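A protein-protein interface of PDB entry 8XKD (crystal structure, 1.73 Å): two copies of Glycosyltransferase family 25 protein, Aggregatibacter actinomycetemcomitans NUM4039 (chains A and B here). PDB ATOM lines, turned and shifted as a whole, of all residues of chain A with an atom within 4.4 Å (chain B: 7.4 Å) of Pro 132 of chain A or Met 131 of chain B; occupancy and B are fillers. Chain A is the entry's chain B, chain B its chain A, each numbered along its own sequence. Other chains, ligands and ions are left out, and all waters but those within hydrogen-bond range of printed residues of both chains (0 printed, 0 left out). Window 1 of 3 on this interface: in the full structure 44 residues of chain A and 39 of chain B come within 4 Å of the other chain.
SD of Met 131 of chain B sits close to SD of Met 131 of chain A (3.7 Å). The backbone carbonyl oxygen (O) of Val 133 of chain A lies close to the side-chain sulfur (SD) of Met 131 of chain B (3.7 Å).
The backbone carbonyl oxygen of Pro 132 of chain B is in hydrogen-bond range of the backbone NH of Lys 155 of chain B, 2.9 Å away. The side-chain amide nitrogen (NE2) of Gln 134 of chain A sits at hydrogen-bond distance from the backbone carbonyl oxygen (O) of Met 131 of chain A.
Pro 132 of chain A touches Met 131 of chain B (CD to CE, 3.7 Å). CZ of Phe 129 of chain B touches CG2 of Val 133 of chain A (3.8 Å). CG2 of Val 133 of chain A touches CD of Pro 132 of chain B, at 3.2 Å. CZ of Phe 157 of chain B touches CG2 of Val 133 of chain A, 3.9 Å away. Val 133 of chain B touches Phe 157 of chain A.
Of chain B, only Met 131 (3.7 Å) comes within 4 Å of Pro 132 of chain A. Printed residues of chain B within 4 Å of Val 133 of chain A: Phe 129 (3.8 Å), Met 131 (3.6 Å), Pro 132 (3.2 Å) and Phe 157 (3.9 Å). Of the printed residues of chain B, Phe 157 of chain A touches Val 133. Printed residues of chain A within 4 Å of Phe 129 of chain B: Val 133 (3.8 Å). Of chain A, only Met 131 (3.3 Å), Pro 132 (3.7 Å) and Val 133 (3.6 Å) come within 4 Å of Met 131 of chain B. The nearest residue of chain B that does not touch Pro 132 of chain A is Pro 132 of chain B (4.3 Å). The nearest printed residue of chain B that does not touch Phe 157 of chain A is Gln 134 of chain B (6.6 Å).
Of the 14 printed residues of chain B, 5 touch a printed residue of chain A. Printed residues of chain B that touch a printed residue of chain A: Phe 129, Met 131, Pro 132, Val 133 and Phe 157. Hydrophobic or aromatic side chains of chain B that line the printed part of chain A: Phe 129, Met 131, Pro 132, Val 133 and Phe 157. Printed residues of chain A that touch a printed residue of chain B: Met 131, Pro 132, Val 133 and Phe 157. Hydrophobic or aromatic side chains of chain A that line the printed part of chain B: Met 131, Pro 132, Val 133 and Phe 157.
Met 131 of chain A touches its own counterpart, Met 131 of chain B. Pro 132 of chain A touches Met 131 of chain B, but with the chains exchanged Met 131 of chain A does not touch Pro 132 of chain B (6.8 Å). Val 133 of chain A touches Pro 132 of chain B, but with the chains exchanged Pro 132 of chain A does not touch Val 133 of chain B (4.3 Å). Val 133 of chain A touches Phe 157 of chain B, and with the chains exchanged Phe 157 of chain A touches Val 133 of chain B. 8 positions are printed for both chains.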
ATOM      1  N   LEU A 130      -3.116 -31.456  30.337  1.00  0.00           N
ATOM      2  CA  LEU A 130      -1.798 -31.749  29.795  1.00  0.00           C
ATOM      3  C   LEU A 130      -1.692 -31.025  28.452  1.00  0.00           C
ATOM      4  O   LEU A 130      -2.604 -31.095  27.628  1.00  0.00           O
ATOM      5  CB  LEU A 130      -1.638 -33.260  29.557  1.00  0.00           C
ATOM      6  CG  LEU A 130      -1.921 -34.234  30.704  1.00  0.00           C
ATOM      7  CD1 LEU A 130      -1.912 -35.671  30.186  1.00  0.00           C
ATOM      8  CD2 LEU A 130      -0.930 -34.056  31.850  1.00  0.00           C
ATOM      9  N   MET A 131      -0.556 -30.368  28.216  1.00  0.00           N
ATOM     10  CA  MET A 131      -0.279 -29.729  26.918  1.00  0.00           C
ATOM     11  C   MET A 131      -0.273 -30.787  25.808  1.00  0.00           C
ATOM     12  O   MET A 131       0.445 -31.772  25.923  1.00  0.00           O
ATOM     13  CB  MET A 131       1.072 -29.005  26.968  1.00  0.00           C
ATOM     14  CG  MET A 131       1.180 -27.835  27.957  1.00  0.00           C
ATOM     15  SD  MET A 131      -0.068 -26.521  27.874  1.00  0.00           S
ATOM     16  CE  MET A 131       0.628 -25.301  28.987  1.00  0.00           C
ATOM     17  N   PRO A 132      -1.092 -30.611  24.745  1.00  0.00           N
ATOM     18  CA  PRO A 132      -1.236 -31.676  23.727  1.00  0.00           C
ATOM     19  C   PRO A 132      -0.070 -31.827  22.750  1.00  0.00           C
ATOM     20  O   PRO A 132      -0.060 -32.748  21.935  1.00  0.00           O
ATOM     21  CB  PRO A 132      -2.473 -31.235  22.933  1.00  0.00           C
ATOM     22  CG  PRO A 132      -2.479 -29.750  23.066  1.00  0.00           C
ATOM     23  CD  PRO A 132      -1.990 -29.474  24.467  1.00  0.00           C
ATOM     24  N   VAL A 133       0.867 -30.887  22.796  1.00  0.00           N
ATOM     25  CA  VAL A 133       2.051 -30.898  21.957  1.00  0.00           C
ATOM     26  C   VAL A 133       3.183 -30.380  22.827  1.00  0.00           C
ATOM     27  O   VAL A 133       3.035 -29.384  23.547  1.00  0.00           O
ATOM     28  CB  VAL A 133       1.899 -30.043  20.676  1.00  0.00           C
ATOM     29  CG1 VAL A 133       0.948 -30.714  19.689  1.00  0.00           C
ATOM     30  CG2 VAL A 133       1.430 -28.637  20.987  1.00  0.00           C
ATOM     31  N   GLN A 134       4.304 -31.094  22.789  1.00  0.00           N
ATOM     32  CA  GLN A 134       5.458 -30.785  23.606  1.00  0.00           C
ATOM     33  C   GLN A 134       6.691 -30.726  22.719  1.00  0.00           C
ATOM     34  O   GLN A 134       6.712 -31.275  21.613  1.00  0.00           O
ATOM     35  CB  GLN A 134       5.671 -31.874  24.659  1.00  0.00           C
ATOM     36  CG  GLN A 134       4.569 -31.971  25.704  1.00  0.00           C
ATOM     37  CD  GLN A 134       3.491 -32.986  25.352  1.00  0.00           C
ATOM     38  OE1 GLN A 134       3.458 -33.539  24.247  1.00  0.00           O
ATOM     39  NE2 GLN A 134       2.601 -33.240  26.301  1.00  0.00           N
ATOM     40  N   THR A 153       6.100 -32.815  19.164  1.00  0.00           N
ATOM     41  CA  THR A 153       5.472 -34.131  19.255  1.00  0.00           C
ATOM     42  C   THR A 153       4.183 -34.034  20.021  1.00  0.00           C
ATOM     43  O   THR A 153       4.076 -33.237  20.939  1.00  0.00           O
ATOM     44  CB  THR A 153       6.385 -35.186  19.931  1.00  0.00           C
ATOM     45  OG1 THR A 153       5.776 -36.470  19.794  1.00  0.00           O
ATOM     46  CG2 THR A 153       6.612 -34.885  21.408  1.00  0.00           C
ATOM     47  N   SER A 154       3.207 -34.871  19.681  1.00  0.00           N
ATOM     48  CA  SER A 154       1.891 -34.831  20.338  1.00  0.00           C
ATOM     49  C   SER A 154       1.906 -35.190  21.839  1.00  0.00           C
ATOM     50  O   SER A 154       2.024 -36.353  22.225  1.00  0.00           O
ATOM     51  CB  SER A 154       0.914 -35.735  19.608  1.00  0.00           C
ATOM     52  OG  SER A 154       1.343 -37.081  19.674  1.00  0.00           O
ATOM     53  N   PHE A 157      -3.527 -35.807  24.906  1.00  0.00           N
ATOM     54  CA  PHE A 157      -4.277 -34.907  25.781  1.00  0.00           C
ATOM     55  C   PHE A 157      -4.948 -35.652  26.941  1.00  0.00           C
ATOM     56  O   PHE A 157      -5.145 -35.104  28.028  1.00  0.00           O
ATOM     57  CB  PHE A 157      -5.355 -34.177  24.996  1.00  0.00           C
ATOM     58  CG  PHE A 157      -5.407 -32.709  25.269  1.00  0.00           C
ATOM     59  CD1 PHE A 157      -5.521 -32.220  26.568  1.00  0.00           C
ATOM     60  CD2 PHE A 157      -5.372 -31.810  24.217  1.00  0.00           C
ATOM     61  CE1 PHE A 157      -5.550 -30.861  26.807  1.00  0.00           C
ATOM     62  CE2 PHE A 157      -5.418 -30.446  24.447  1.00  0.00           C
ATOM     63  CZ  PHE A 157      -5.525 -29.975  25.740  1.00  0.00           C
ATOM     64  N   THR B 128       9.055 -18.336  18.148  1.00  0.00           N
ATOM     65  CA  THR B 128       8.712 -18.926  19.449  1.00  0.00           C
ATOM     66  C   THR B 128       7.589 -19.967  19.364  1.00  0.00           C
ATOM     67  O   THR B 128       6.652 -19.858  18.558  1.00  0.00           O
ATOM     68  CB  THR B 128       8.324 -17.834  20.441  1.00  0.00           C
ATOM     69  OG1 THR B 128       7.259 -17.069  19.879  1.00  0.00           O
ATOM     70  CG2 THR B 128       9.514 -16.910  20.693  1.00  0.00           C
ATOM     71  N   PHE B 129       7.751 -21.040  20.135  1.00  0.00           N
ATOM     72  CA  PHE B 129       6.739 -22.081  20.192  1.00  0.00           C
ATOM     73  C   PHE B 129       5.531 -21.563  20.977  1.00  0.00           C
ATOM     74  O   PHE B 129       5.706 -21.039  22.070  1.00  0.00           O
ATOM     75  CB  PHE B 129       7.320 -23.319  20.870  1.00  0.00           C
ATOM     76  CG  PHE B 129       6.315 -24.399  21.097  1.00  0.00           C
ATOM     77  CD1 PHE B 129       5.806 -25.132  20.035  1.00  0.00           C
ATOM     78  CD2 PHE B 129       5.874 -24.690  22.383  1.00  0.00           C
ATOM     79  CE1 PHE B 129       4.873 -26.131  20.255  1.00  0.00           C
ATOM     80  CE2 PHE B 129       4.936 -25.676  22.599  1.00  0.00           C
ATOM     81  CZ  PHE B 129       4.432 -26.391  21.541  1.00  0.00           C
ATOM     82  N   LEU B 130       4.341 -21.687  20.397  1.00  0.00           N
ATOM     83  CA  LEU B 130       3.092 -21.241  21.050  1.00  0.00           C
ATOM     84  C   LEU B 130       2.182 -22.450  21.297  1.00  0.00           C
ATOM     85  O   LEU B 130       1.934 -23.214  20.369  1.00  0.00           O
ATOM     86  CB  LEU B 130       2.366 -20.218  20.161  1.00  0.00           C
ATOM     87  CG  LEU B 130       3.180 -19.010  19.647  1.00  0.00           C
ATOM     88  CD1 LEU B 130       2.429 -18.245  18.559  1.00  0.00           C
ATOM     89  CD2 LEU B 130       3.565 -18.083  20.803  1.00  0.00           C
ATOM     90  N   MET B 131       1.737 -22.648  22.534  1.00  0.00           N
ATOM     91  CA  MET B 131       0.841 -23.770  22.864  1.00  0.00           C
ATOM     92  C   MET B 131      -0.484 -23.612  22.105  1.00  0.00           C
ATOM     93  O   MET B 131      -1.101 -22.564  22.182  1.00  0.00           O
ATOM     94  CB  MET B 131       0.573 -23.814  24.371  1.00  0.00           C
ATOM     95  CG  MET B 131       1.729 -24.338  25.213  1.00  0.00           C
ATOM     96  SD  MET B 131       2.193 -26.075  24.954  1.00  0.00           S
ATOM     97  CE  MET B 131       0.659 -26.869  24.469  1.00  0.00           C
ATOM     98  N   PRO B 132      -0.927 -24.646  21.359  1.00  0.00           N
ATOM     99  CA  PRO B 132      -2.169 -24.511  20.591  1.00  0.00           C
ATOM    100  C   PRO B 132      -3.474 -24.597  21.391  1.00  0.00           C
ATOM    101  O   PRO B 132      -4.545 -24.387  20.816  1.00  0.00           O
ATOM    102  CB  PRO B 132      -2.103 -25.677  19.595  1.00  0.00           C
ATOM    103  CG  PRO B 132      -1.308 -26.700  20.309  1.00  0.00           C
ATOM    104  CD  PRO B 132      -0.277 -25.940  21.101  1.00  0.00           C
ATOM    105  N   VAL B 133      -3.386 -24.929  22.674  1.00  0.00           N
ATOM    106  CA  VAL B 133      -4.571 -24.926  23.554  1.00  0.00           C
ATOM    107  C   VAL B 133      -4.178 -24.356  24.904  1.00  0.00           C
ATOM    108  O   VAL B 133      -3.140 -24.725  25.434  1.00  0.00           O
ATOM    109  CB  VAL B 133      -5.174 -26.339  23.711  1.00  0.00           C
ATOM    110  CG1 VAL B 133      -6.358 -26.314  24.682  1.00  0.00           C
ATOM    111  CG2 VAL B 133      -5.611 -26.876  22.352  1.00  0.00           C
ATOM    112  N   GLN B 134      -4.985 -23.434  25.428  1.00  0.00           N
ATOM    113  CA  GLN B 134      -4.716 -22.803  26.717  1.00  0.00           C
ATOM    114  C   GLN B 134      -5.957 -22.839  27.597  1.00  0.00           C
ATOM    115  O   GLN B 134      -7.063 -22.845  27.088  1.00  0.00           O
ATOM    116  CB  GLN B 134      -4.347 -21.333  26.551  1.00  0.00           C
ATOM    117  CG  GLN B 134      -3.081 -21.059  25.760  1.00  0.00           C
ATOM    118  CD  GLN B 134      -2.610 -19.617  25.905  1.00  0.00           C
ATOM    119  OE1 GLN B 134      -3.360 -18.736  26.350  1.00  0.00           O
ATOM    120  NE2 GLN B 134      -1.362 -19.369  25.531  1.00  0.00           N
ATOM    121  N   THR B 153      -9.370 -23.120  25.322  1.00  0.00           N
ATOM    122  CA  THR B 153      -9.440 -22.277  24.125  1.00  0.00           C
ATOM    123  C   THR B 153      -8.245 -22.597  23.213  1.00  0.00           C
ATOM    124  O   THR B 153      -7.179 -22.980  23.689  1.00  0.00           O
ATOM    125  CB  THR B 153      -9.386 -20.809  24.504  1.00  0.00           C
ATOM    126  OG1 THR B 153      -8.104 -20.505  25.075  1.00  0.00           O
ATOM    127  CG2 THR B 153     -10.445 -20.486  25.523  1.00  0.00           C
ATOM    128  N   SER B 154      -8.466 -22.455  21.919  1.00  0.00           N
ATOM    129  CA  SER B 154      -7.446 -22.777  20.919  1.00  0.00           C
ATOM    130  C   SER B 154      -6.669 -21.510  20.594  1.00  0.00           C
ATOM    131  O   SER B 154      -7.175 -20.376  20.724  1.00  0.00           O
ATOM    132  CB  SER B 154      -8.087 -23.361  19.658  1.00  0.00           C
ATOM    133  OG  SER B 154      -8.977 -22.426  19.065  1.00  0.00           O
ATOM    134  N   LYS B 155      -5.413 -21.715  20.231  1.00  0.00           N
ATOM    135  CA  LYS B 155      -4.511 -20.639  19.848  1.00  0.00           C
ATOM    136  C   LYS B 155      -3.859 -21.132  18.574  1.00  0.00           C
ATOM    137  O   LYS B 155      -3.677 -22.340  18.410  1.00  0.00           O
ATOM    138  CB  LYS B 155      -3.427 -20.409  20.903  1.00  0.00           C
ATOM    139  CG  LYS B 155      -3.927 -19.950  22.268  1.00  0.00           C
ATOM    140  CD  LYS B 155      -4.515 -18.545  22.224  1.00  0.00           C
ATOM    141  CE  LYS B 155      -5.200 -18.191  23.532  1.00  0.00           C
ATOM    142  NZ  LYS B 155      -6.029 -16.963  23.383  1.00  0.00           N
ATOM    143  N   HIS B 156      -3.530 -20.220  17.671  1.00  0.00           N
ATOM    144  CA  HIS B 156      -2.929 -20.638  16.418  1.00  0.00           C
ATOM    145  C   HIS B 156      -1.411 -20.725  16.629  1.00  0.00           C
ATOM    146  O   HIS B 156      -0.827 -19.944  17.372  1.00  0.00           O
ATOM    147  CB  HIS B 156      -3.304 -19.692  15.270  1.00  0.00           C
ATOM    148  CG  HIS B 156      -4.708 -19.870  14.757  1.00  0.00           C
ATOM    149  ND1 HIS B 156      -5.732 -19.001  15.077  1.00  0.00           N
ATOM    150  CD2 HIS B 156      -5.251 -20.797  13.928  1.00  0.00           C
ATOM    151  CE1 HIS B 156      -6.843 -19.388  14.474  1.00  0.00           C
ATOM    152  NE2 HIS B 156      -6.581 -20.478  13.774  1.00  0.00           N
ATOM    153  N   PHE B 157      -0.787 -21.720  16.010  1.00  0.00           N
ATOM    154  CA  PHE B 157       0.641 -21.757  15.893  1.00  0.00           C
ATOM    155  C   PHE B 157       0.947 -20.633  14.904  1.00  0.00           C
ATOM    156  O   PHE B 157       0.213 -20.414  13.961  1.00  0.00           O
ATOM    157  CB  PHE B 157       1.085 -23.073  15.279  1.00  0.00           C
ATOM    158  CG  PHE B 157       1.424 -24.126  16.277  1.00  0.00           C
ATOM    159  CD1 PHE B 157       2.493 -23.938  17.133  1.00  0.00           C
ATOM    160  CD2 PHE B 157       0.694 -25.310  16.342  1.00  0.00           C
ATOM    161  CE1 PHE B 157       2.838 -24.921  18.043  1.00  0.00           C
ATOM    162  CE2 PHE B 157       1.026 -26.294  17.254  1.00  0.00           C
ATOM    163  CZ  PHE B 157       2.090 -26.090  18.127  1.00  0.00           C
ATOM    164  N   ASN B 193      -0.300 -28.837  13.346  1.00  0.00           N
ATOM    165  CA  ASN B 193      -1.184 -29.549  14.298  1.00  0.00           C
ATOM    166  C   ASN B 193      -1.570 -30.870  13.645  1.00  0.00           C
ATOM    167  O   ASN B 193      -1.000 -31.924  13.971  1.00  0.00           O
ATOM    168  CB  ASN B 193      -2.400 -28.670  14.639  1.00  0.00           C
ATOM    169  CG  ASN B 193      -2.816 -28.728  16.122  1.00  0.00           C
ATOM    170  OD1 ASN B 193      -2.089 -29.224  16.989  1.00  0.00           O
ATOM    171  ND2 ASN B 193      -3.992 -28.181  16.411  1.00  0.00           N
ATOM    172  N   ILE B 196       1.370 -33.223  12.253  1.00  0.00           N
ATOM    173  CA  ILE B 196       2.432 -33.662  13.161  1.00  0.00           C
ATOM    174  C   ILE B 196       2.533 -35.189  13.248  1.00  0.00           C
ATOM    175  O   ILE B 196       3.642 -35.720  13.395  1.00  0.00           O
ATOM    176  CB  ILE B 196       2.261 -33.053  14.586  1.00  0.00           C
ATOM    177  CG1 ILE B 196       2.382 -31.523  14.542  1.00  0.00           C
ATOM    178  CG2 ILE B 196       3.290 -33.597  15.581  1.00  0.00           C
ATOM    179  CD1 ILE B 196       3.706 -31.011  14.008  1.00  0.00           C
